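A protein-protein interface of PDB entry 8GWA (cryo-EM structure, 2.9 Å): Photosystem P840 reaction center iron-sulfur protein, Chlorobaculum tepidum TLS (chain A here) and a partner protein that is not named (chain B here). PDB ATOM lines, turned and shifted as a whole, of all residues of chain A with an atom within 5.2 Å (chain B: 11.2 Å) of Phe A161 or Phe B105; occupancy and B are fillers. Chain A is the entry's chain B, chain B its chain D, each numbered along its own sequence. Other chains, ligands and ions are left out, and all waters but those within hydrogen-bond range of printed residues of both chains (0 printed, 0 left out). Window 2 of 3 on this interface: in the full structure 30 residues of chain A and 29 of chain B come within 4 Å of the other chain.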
ATOM      1  N   TYR A 159      -8.606 -19.327  11.789  1.00  0.00           N
ATOM      2  CA  TYR A 159     -10.059 -19.396  11.783  1.00  0.00           C
ATOM      3  C   TYR A 159     -10.543 -20.645  12.508  1.00  0.00           C
ATOM      4  O   TYR A 159      -9.937 -21.716  12.395  1.00  0.00           O
ATOM      5  CB  TYR A 159     -10.596 -19.396  10.348  1.00  0.00           C
ATOM      6  CG  TYR A 159     -10.936 -18.026   9.810  1.00  0.00           C
ATOM      7  CD1 TYR A 159     -10.039 -17.326   9.014  1.00  0.00           C
ATOM      8  CD2 TYR A 159     -12.162 -17.441  10.083  1.00  0.00           C
ATOM      9  CE1 TYR A 159     -10.352 -16.077   8.517  1.00  0.00           C
ATOM     10  CE2 TYR A 159     -12.482 -16.195   9.590  1.00  0.00           C
ATOM     11  CZ  TYR A 159     -11.575 -15.517   8.808  1.00  0.00           C
ATOM     12  OH  TYR A 159     -11.896 -14.274   8.318  1.00  0.00           O
ATOM     13  N   LYS A 160     -11.636 -20.498  13.255  1.00  0.00           N
ATOM     14  CA  LYS A 160     -12.397 -21.621  13.783  1.00  0.00           C
ATOM     15  C   LYS A 160     -13.857 -21.412  13.412  1.00  0.00           C
ATOM     16  O   LYS A 160     -14.352 -20.281  13.431  1.00  0.00           O
ATOM     17  CB  LYS A 160     -12.239 -21.764  15.305  1.00  0.00           C
ATOM     18  CG  LYS A 160     -12.616 -20.532  16.107  1.00  0.00           C
ATOM     19  CD  LYS A 160     -12.343 -20.744  17.588  1.00  0.00           C
ATOM     20  CE  LYS A 160     -13.492 -21.470  18.268  1.00  0.00           C
ATOM     21  NZ  LYS A 160     -14.588 -20.543  18.657  1.00  0.00           N
ATOM     22  N   PHE A 161     -14.548 -22.500  13.070  1.00  0.00           N
ATOM     23  CA  PHE A 161     -15.849 -22.402  12.423  1.00  0.00           C
ATOM     24  C   PHE A 161     -16.997 -22.857  13.317  1.00  0.00           C
ATOM     25  O   PHE A 161     -17.938 -22.094  13.540  1.00  0.00           O
ATOM     26  CB  PHE A 161     -15.827 -23.210  11.122  1.00  0.00           C
ATOM     27  CG  PHE A 161     -14.819 -22.715  10.128  1.00  0.00           C
ATOM     28  CD1 PHE A 161     -15.090 -21.614   9.336  1.00  0.00           C
ATOM     29  CD2 PHE A 161     -13.593 -23.343   9.997  1.00  0.00           C
ATOM     30  CE1 PHE A 161     -14.161 -21.155   8.429  1.00  0.00           C
ATOM     31  CE2 PHE A 161     -12.661 -22.888   9.089  1.00  0.00           C
ATOM     32  CZ  PHE A 161     -12.946 -21.792   8.304  1.00  0.00           C
ATOM     33  N   TYR A 162     -16.967 -24.097  13.801  1.00  0.00           N
ATOM     34  CA  TYR A 162     -17.938 -24.607  14.767  1.00  0.00           C
ATOM     35  C   TYR A 162     -19.394 -24.496  14.316  1.00  0.00           C
ATOM     36  O   TYR A 162     -20.306 -24.769  15.103  1.00  0.00           O
ATOM     37  CB  TYR A 162     -17.739 -23.925  16.133  1.00  0.00           C
ATOM     38  CG  TYR A 162     -18.209 -22.488  16.307  1.00  0.00           C
ATOM     39  CD1 TYR A 162     -19.559 -22.163  16.382  1.00  0.00           C
ATOM     40  CD2 TYR A 162     -17.287 -21.458  16.442  1.00  0.00           C
ATOM     41  CE1 TYR A 162     -19.974 -20.857  16.553  1.00  0.00           C
ATOM     42  CE2 TYR A 162     -17.693 -20.150  16.612  1.00  0.00           C
ATOM     43  CZ  TYR A 162     -19.037 -19.855  16.670  1.00  0.00           C
ATOM     44  OH  TYR A 162     -19.448 -18.554  16.842  1.00  0.00           O
ATOM     45  N   GLY A 163     -19.632 -24.131  13.064  1.00  0.00           N
ATOM     46  CA  GLY A 163     -20.995 -23.998  12.589  1.00  0.00           C
ATOM     47  C   GLY A 163     -21.040 -23.167  11.320  1.00  0.00           C
ATOM     48  O   GLY A 163     -20.037 -23.017  10.624  1.00  0.00           O
ATOM     49  N   ASP A 164     -22.226 -22.634  11.044  1.00  0.00           N
ATOM     50  CA  ASP A 164     -22.417 -21.804   9.866  1.00  0.00           C
ATOM     51  C   ASP A 164     -21.841 -20.414  10.094  1.00  0.00           C
ATOM     52  O   ASP A 164     -21.862 -19.879  11.206  1.00  0.00           O
ATOM     53  CB  ASP A 164     -23.899 -21.706   9.501  1.00  0.00           C
ATOM     54  CG  ASP A 164     -24.711 -20.952  10.535  1.00  0.00           C
ATOM     55  OD1 ASP A 164     -24.328 -20.962  11.723  1.00  0.00           O
ATOM     56  OD2 ASP A 164     -25.733 -20.344  10.156  1.00  0.00           O
ATOM     57  N   VAL A 165     -21.310 -19.832   9.017  1.00  0.00           N
ATOM     58  CA  VAL A 165     -20.690 -18.515   9.097  1.00  0.00           C
ATOM     59  C   VAL A 165     -21.707 -17.390   9.000  1.00  0.00           C
ATOM     60  O   VAL A 165     -21.368 -16.232   9.290  1.00  0.00           O
ATOM     61  CB  VAL A 165     -19.623 -18.371   7.999  1.00  0.00           C
ATOM     62  CG1 VAL A 165     -18.630 -19.514   8.099  1.00  0.00           C
ATOM     63  CG2 VAL A 165     -20.276 -18.353   6.644  1.00  0.00           C
ATOM     64  N   GLY A 169     -20.263 -17.774  13.012  1.00  0.00           N
ATOM     65  CA  GLY A 169     -19.526 -18.979  13.328  1.00  0.00           C
ATOM     66  C   GLY A 169     -18.257 -19.103  12.513  1.00  0.00           C
ATOM     67  O   GLY A 169     -18.011 -20.137  11.891  1.00  0.00           O
ATOM     68  N   PHE A 170     -17.482 -18.028  12.442  1.00  0.00           N
ATOM     69  CA  PHE A 170     -16.165 -18.060  11.813  1.00  0.00           C
ATOM     70  C   PHE A 170     -15.191 -17.163  12.575  1.00  0.00           C
ATOM     71  O   PHE A 170     -14.448 -16.373  11.991  1.00  0.00           O
ATOM     72  CB  PHE A 170     -16.283 -17.724  10.325  1.00  0.00           C
ATOM     73  CG  PHE A 170     -16.811 -16.350  10.037  1.00  0.00           C
ATOM     74  CD1 PHE A 170     -18.166 -16.088  10.125  1.00  0.00           C
ATOM     75  CD2 PHE A 170     -15.973 -15.350   9.586  1.00  0.00           C
ATOM     76  CE1 PHE A 170     -18.664 -14.839   9.839  1.00  0.00           C
ATOM     77  CE2 PHE A 170     -16.471 -14.101   9.288  1.00  0.00           C
ATOM     78  CZ  PHE A 170     -17.817 -13.847   9.417  1.00  0.00           C
ATOM     79  N   GLU B  98     -15.515 -25.906  24.002  1.00  0.00           N
ATOM     80  CA  GLU B  98     -15.545 -25.824  22.550  1.00  0.00           C
ATOM     81  C   GLU B  98     -15.559 -27.199  21.897  1.00  0.00           C
ATOM     82  O   GLU B  98     -16.080 -27.338  20.789  1.00  0.00           O
ATOM     83  CB  GLU B  98     -14.350 -25.019  22.035  1.00  0.00           C
ATOM     84  CG  GLU B  98     -14.185 -23.653  22.682  1.00  0.00           C
ATOM     85  CD  GLU B  98     -15.273 -22.676  22.279  1.00  0.00           C
ATOM     86  OE1 GLU B  98     -15.594 -22.606  21.074  1.00  0.00           O
ATOM     87  OE2 GLU B  98     -15.809 -21.979  23.165  1.00  0.00           O
ATOM     88  N   ASN B  99     -15.032 -28.222  22.572  1.00  0.00           N
ATOM     89  CA  ASN B  99     -15.053 -29.569  22.015  1.00  0.00           C
ATOM     90  C   ASN B  99     -16.467 -30.111  21.866  1.00  0.00           C
ATOM     91  O   ASN B  99     -16.655 -31.128  21.190  1.00  0.00           O
ATOM     92  CB  ASN B  99     -14.225 -30.507  22.893  1.00  0.00           C
ATOM     93  CG  ASN B  99     -12.734 -30.340  22.676  1.00  0.00           C
ATOM     94  OD1 ASN B  99     -12.297 -29.856  21.632  1.00  0.00           O
ATOM     95  ND2 ASN B  99     -11.945 -30.740  23.665  1.00  0.00           N
ATOM     96  N   ARG B 100     -17.455 -29.461  22.481  1.00  0.00           N
ATOM     97  CA  ARG B 100     -18.847 -29.858  22.313  1.00  0.00           C
ATOM     98  C   ARG B 100     -19.399 -29.458  20.952  1.00  0.00           C
ATOM     99  O   ARG B 100     -20.273 -30.149  20.419  1.00  0.00           O
ATOM    100  CB  ARG B 100     -19.701 -29.234  23.415  1.00  0.00           C
ATOM    101  CG  ARG B 100     -19.305 -29.648  24.815  1.00  0.00           C
ATOM    102  CD  ARG B 100     -20.045 -28.838  25.865  1.00  0.00           C
ATOM    103  NE  ARG B 100     -21.452 -29.207  25.968  1.00  0.00           N
ATOM    104  CZ  ARG B 100     -22.443 -28.556  25.377  1.00  0.00           C
ATOM    105  NH1 ARG B 100     -22.222 -27.485  24.633  1.00  0.00           N
ATOM    106  NH2 ARG B 100     -23.690 -28.989  25.539  1.00  0.00           N
ATOM    107  N   TYR B 101     -18.915 -28.352  20.379  1.00  0.00           N
ATOM    108  CA  TYR B 101     -19.522 -27.823  19.164  1.00  0.00           C
ATOM    109  C   TYR B 101     -18.520 -27.297  18.141  1.00  0.00           C
ATOM    110  O   TYR B 101     -18.944 -26.685  17.154  1.00  0.00           O
ATOM    111  CB  TYR B 101     -20.514 -26.708  19.516  1.00  0.00           C
ATOM    112  CG  TYR B 101     -19.854 -25.424  19.965  1.00  0.00           C
ATOM    113  CD1 TYR B 101     -19.171 -25.354  21.173  1.00  0.00           C
ATOM    114  CD2 TYR B 101     -19.903 -24.285  19.177  1.00  0.00           C
ATOM    115  CE1 TYR B 101     -18.565 -24.184  21.583  1.00  0.00           C
ATOM    116  CE2 TYR B 101     -19.296 -23.113  19.581  1.00  0.00           C
ATOM    117  CZ  TYR B 101     -18.631 -23.067  20.783  1.00  0.00           C
ATOM    118  OH  TYR B 101     -18.029 -21.897  21.182  1.00  0.00           O
ATOM    119  N   VAL B 102     -17.220 -27.511  18.325  1.00  0.00           N
ATOM    120  CA  VAL B 102     -16.207 -27.018  17.397  1.00  0.00           C
ATOM    121  C   VAL B 102     -15.449 -28.208  16.827  1.00  0.00           C
ATOM    122  O   VAL B 102     -14.977 -29.068  17.580  1.00  0.00           O
ATOM    123  CB  VAL B 102     -15.230 -26.034  18.069  1.00  0.00           C
ATOM    124  CG1 VAL B 102     -14.324 -25.397  17.028  1.00  0.00           C
ATOM    125  CG2 VAL B 102     -15.979 -24.968  18.850  1.00  0.00           C
ATOM    126  N   ILE B 103     -15.332 -28.253  15.502  1.00  0.00           N
ATOM    127  CA  ILE B 103     -14.510 -29.238  14.811  1.00  0.00           C
ATOM    128  C   ILE B 103     -13.206 -28.569  14.409  1.00  0.00           C
ATOM    129  O   ILE B 103     -13.212 -27.529  13.738  1.00  0.00           O
ATOM    130  CB  ILE B 103     -15.236 -29.818  13.585  1.00  0.00           C
ATOM    131  CG1 ILE B 103     -16.535 -30.504  14.007  1.00  0.00           C
ATOM    132  CG2 ILE B 103     -14.337 -30.794  12.847  1.00  0.00           C
ATOM    133  CD1 ILE B 103     -17.392 -30.942  12.846  1.00  0.00           C
ATOM    134  N   ASP B 104     -12.084 -29.164  14.816  1.00  0.00           N
ATOM    135  CA  ASP B 104     -10.764 -28.572  14.600  1.00  0.00           C
ATOM    136  C   ASP B 104     -10.275 -28.903  13.194  1.00  0.00           C
ATOM    137  O   ASP B 104      -9.472 -29.811  12.972  1.00  0.00           O
ATOM    138  CB  ASP B 104      -9.784 -29.055  15.661  1.00  0.00           C
ATOM    139  CG  ASP B 104      -9.941 -28.320  16.971  1.00  0.00           C
ATOM    140  OD1 ASP B 104     -10.357 -27.145  16.940  1.00  0.00           O
ATOM    141  OD2 ASP B 104      -9.650 -28.915  18.030  1.00  0.00           O
ATOM    142  N   PHE B 105     -10.784 -28.144  12.222  1.00  0.00           N
ATOM    143  CA  PHE B 105     -10.192 -28.176  10.889  1.00  0.00           C
ATOM    144  C   PHE B 105      -8.765 -27.649  10.920  1.00  0.00           C
ATOM    145  O   PHE B 105      -7.867 -28.218  10.287  1.00  0.00           O
ATOM    146  CB  PHE B 105     -11.043 -27.367   9.911  1.00  0.00           C
ATOM    147  CG  PHE B 105     -12.472 -27.820   9.827  1.00  0.00           C
ATOM    148  CD1 PHE B 105     -12.780 -29.142   9.553  1.00  0.00           C
ATOM    149  CD2 PHE B 105     -13.509 -26.924  10.017  1.00  0.00           C
ATOM    150  CE1 PHE B 105     -14.093 -29.560   9.470  1.00  0.00           C
ATOM    151  CE2 PHE B 105     -14.823 -27.337   9.938  1.00  0.00           C
ATOM    152  CZ  PHE B 105     -15.115 -28.656   9.664  1.00  0.00           C
ATOM    153  N   ASP B 106      -8.537 -26.560  11.654  1.00  0.00           N
ATOM    154  CA  ASP B 106      -7.208 -25.980  11.802  1.00  0.00           C
ATOM    155  C   ASP B 106      -6.378 -26.663  12.881  1.00  0.00           C
ATOM    156  O   ASP B 106      -5.169 -26.417  12.953  1.00  0.00           O
ATOM    157  CB  ASP B 106      -7.324 -24.486  12.113  1.00  0.00           C
ATOM    158  CG  ASP B 106      -6.262 -23.662  11.413  1.00  0.00           C
ATOM    159  OD1 ASP B 106      -5.302 -24.254  10.877  1.00  0.00           O
ATOM    160  OD2 ASP B 106      -6.389 -22.419  11.398  1.00  0.00           O
ATOM    161  N   LYS B 107      -6.996 -27.494  13.721  1.00  0.00           N
ATOM    162  CA  LYS B 107      -6.374 -28.246  14.809  1.00  0.00           C
ATOM    163  C   LYS B 107      -5.817 -27.357  15.914  1.00  0.00           C
ATOM    164  O   LYS B 107      -5.162 -27.872  16.828  1.00  0.00           O
ATOM    165  CB  LYS B 107      -5.258 -29.178  14.315  1.00  0.00           C
ATOM    166  CG  LYS B 107      -5.739 -30.273  13.381  1.00  0.00           C
ATOM    167  CD  LYS B 107      -6.693 -31.217  14.092  1.00  0.00           C
ATOM    168  CE  LYS B 107      -5.961 -32.067  15.118  1.00  0.00           C
ATOM    169  NZ  LYS B 107      -6.861 -33.053  15.778  1.00  0.00           N
ATOM    170  N   ARG B 108      -6.047 -26.045  15.868  1.00  0.00           N
ATOM    171  CA  ARG B 108      -5.564 -25.154  16.911  1.00  0.00           C
ATOM    172  C   ARG B 108      -6.527 -24.023  17.246  1.00  0.00           C
ATOM    173  O   ARG B 108      -6.178 -23.169  18.068  1.00  0.00           O
ATOM    174  CB  ARG B 108      -4.204 -24.564  16.511  1.00  0.00           C
ATOM    175  CG  ARG B 108      -4.292 -23.636  15.324  1.00  0.00           C
ATOM    176  CD  ARG B 108      -2.948 -23.062  14.935  1.00  0.00           C
ATOM    177  NE  ARG B 108      -3.097 -22.046  13.900  1.00  0.00           N
ATOM    178  CZ  ARG B 108      -2.096 -21.354  13.377  1.00  0.00           C
ATOM    179  NH1 ARG B 108      -0.846 -21.542  13.767  1.00  0.00           N
ATOM    180  NH2 ARG B 108      -2.356 -20.450  12.437  1.00  0.00           N
ATOM    181  N   GLY B 109      -7.715 -23.980  16.641  1.00  0.00           N
ATOM    182  CA  GLY B 109      -8.653 -22.914  16.953  1.00  0.00           C
ATOM    183  C   GLY B 109      -9.180 -22.987  18.372  1.00  0.00           C
ATOM    184  O   GLY B 109      -9.342 -21.961  19.038  1.00  0.00           O
ATOM    185  N   VAL B 110      -9.465 -24.199  18.852  1.00  0.00           N
ATOM    186  CA  VAL B 110      -9.931 -24.368  20.224  1.00  0.00           C
ATOM    187  C   VAL B 110      -8.809 -24.074  21.212  1.00  0.00           C
ATOM    188  O   VAL B 110      -9.040 -23.491  22.279  1.00  0.00           O
ATOM    189  CB  VAL B 110     -10.504 -25.785  20.417  1.00  0.00           C
ATOM    190  CG1 VAL B 110     -10.890 -26.010  21.861  1.00  0.00           C
ATOM    191  CG2 VAL B 110     -11.711 -25.984  19.525  1.00  0.00           C
ATOM    192  N   LYS B 111      -7.580 -24.467  20.873  1.00  0.00           N
ATOM    193  CA  LYS B 111      -6.456 -24.278  21.786  1.00  0.00           C
ATOM    194  C   LYS B 111      -6.233 -22.805  22.100  1.00  0.00           C
ATOM    195  O   LYS B 111      -5.980 -22.440  23.254  1.00  0.00           O
ATOM    196  CB  LYS B 111      -5.191 -24.893  21.189  1.00  0.00           C
ATOM    197  CG  LYS B 111      -4.013 -24.960  22.150  1.00  0.00           C
ATOM    198  CD  LYS B 111      -2.685 -25.144  21.419  1.00  0.00           C
ATOM    199  CE  LYS B 111      -2.811 -26.030  20.185  1.00  0.00           C
ATOM    200  NZ  LYS B 111      -3.344 -27.389  20.495  1.00  0.00           N
ATOM    201  N   THR B 113      -8.405 -20.254  21.885  1.00  0.00           N
ATOM    202  CA  THR B 113      -9.653 -19.528  22.062  1.00  0.00           C
ATOM    203  C   THR B 113      -9.633 -18.787  23.390  1.00  0.00           C
ATOM    204  O   THR B 113      -9.508 -19.404  24.452  1.00  0.00           O
ATOM    205  CB  THR B 113     -10.849 -20.479  22.004  1.00  0.00           C
ATOM    206  OG1 THR B 113     -10.866 -21.144  20.734  1.00  0.00           O
ATOM    207  CG2 THR B 113     -12.150 -19.710  22.188  1.00  0.00           C
ATOM    208  N   ARG B 115     -11.733 -15.508  25.486  1.00  0.00           N
ATOM    209  CA  ARG B 115     -12.960 -14.734  25.459  1.00  0.00           C
ATOM    210  C   ARG B 115     -13.049 -13.913  26.735  1.00  0.00           C
ATOM    211  O   ARG B 115     -12.343 -14.168  27.714  1.00  0.00           O
ATOM    212  CB  ARG B 115     -14.181 -15.647  25.311  1.00  0.00           C
ATOM    213  CG  ARG B 115     -14.205 -16.354  23.970  1.00  0.00           C
ATOM    214  CD  ARG B 115     -15.385 -17.271  23.804  1.00  0.00           C
ATOM    215  NE  ARG B 115     -16.617 -16.502  23.759  1.00  0.00           N
ATOM    216  CZ  ARG B 115     -17.828 -17.032  23.774  1.00  0.00           C
ATOM    217  NH1 ARG B 115     -18.009 -18.337  23.802  1.00  0.00           N
ATOM    218  NH2 ARG B 115     -18.884 -16.233  23.738  1.00  0.00           N
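The side-chain carboxylate (OE1) of Glu B98 is in salt-bridge range of the side-chain amino group (NZ) of Lys A160 (3.3 Å). O of Tyr B101 sits close to O of Tyr A162 (3.1 Å).
The backbone carbonyl oxygen (O) of Val B110 sits at hydrogen-bond distance from the side-chain hydroxyl (OG1) of Thr B113. The side-chain hydroxyl (OG1) of Thr B113 lies within hydrogen-bond range of the backbone carbonyl oxygen (O) of Gly B109 (2.4 Å). The backbone carbonyl oxygen of Gly A169 sits close to the backbone carbonyl oxygen of Phe A161. OE1 of Glu B98 lies within hydrogen-bond range of OH of Tyr B101, at 2.5 Å.
Phe A161 touches just one residue of chain B: Phe B105 (3.6 Å). Phe B105 touches just one residue of chain A: Phe A161. Of chain B, only Tyr B101 and Val B102 come within 4 Å of Tyr A162. Of the printed residues of chain A, Thr B113 touches Lys A160. Printed residues of chain A within 4 Å of Glu B98: Lys A160. Of the printed residues of chain A, Asp B106 touches Tyr A159. Printed residues of chain A within 4 Å of Gly B109: Lys A160 (3.5 Å). The nearest residue of chain B that does not touch Phe A161 is Val B102 (4.9 Å). The nearest printed residue of chain A that does not touch Phe B105 is Tyr A162 (5.5 Å).
Of the 16 printed residues of chain B, 7 touch a printed residue of chain A. Hydrophobic or aromatic side chains of chain B within 4 Å of the printed part of chain A: Tyr B101, Val B102 and Phe B105. Hydrophobic or aromatic side chains of chain A that line the printed part of chain B: Phe A161 and Tyr A162.
Tyr A159 touches Asp B106 (O to OD2, 3.8 Å). Lys A160 touches Gly B109. Lys A160 touches Thr B113. Phe A161 touches Phe B105 (CD2 to CD2, 3.6 Å). CB of Tyr A162 touches CG2 of Val B102 (3.4 Å).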
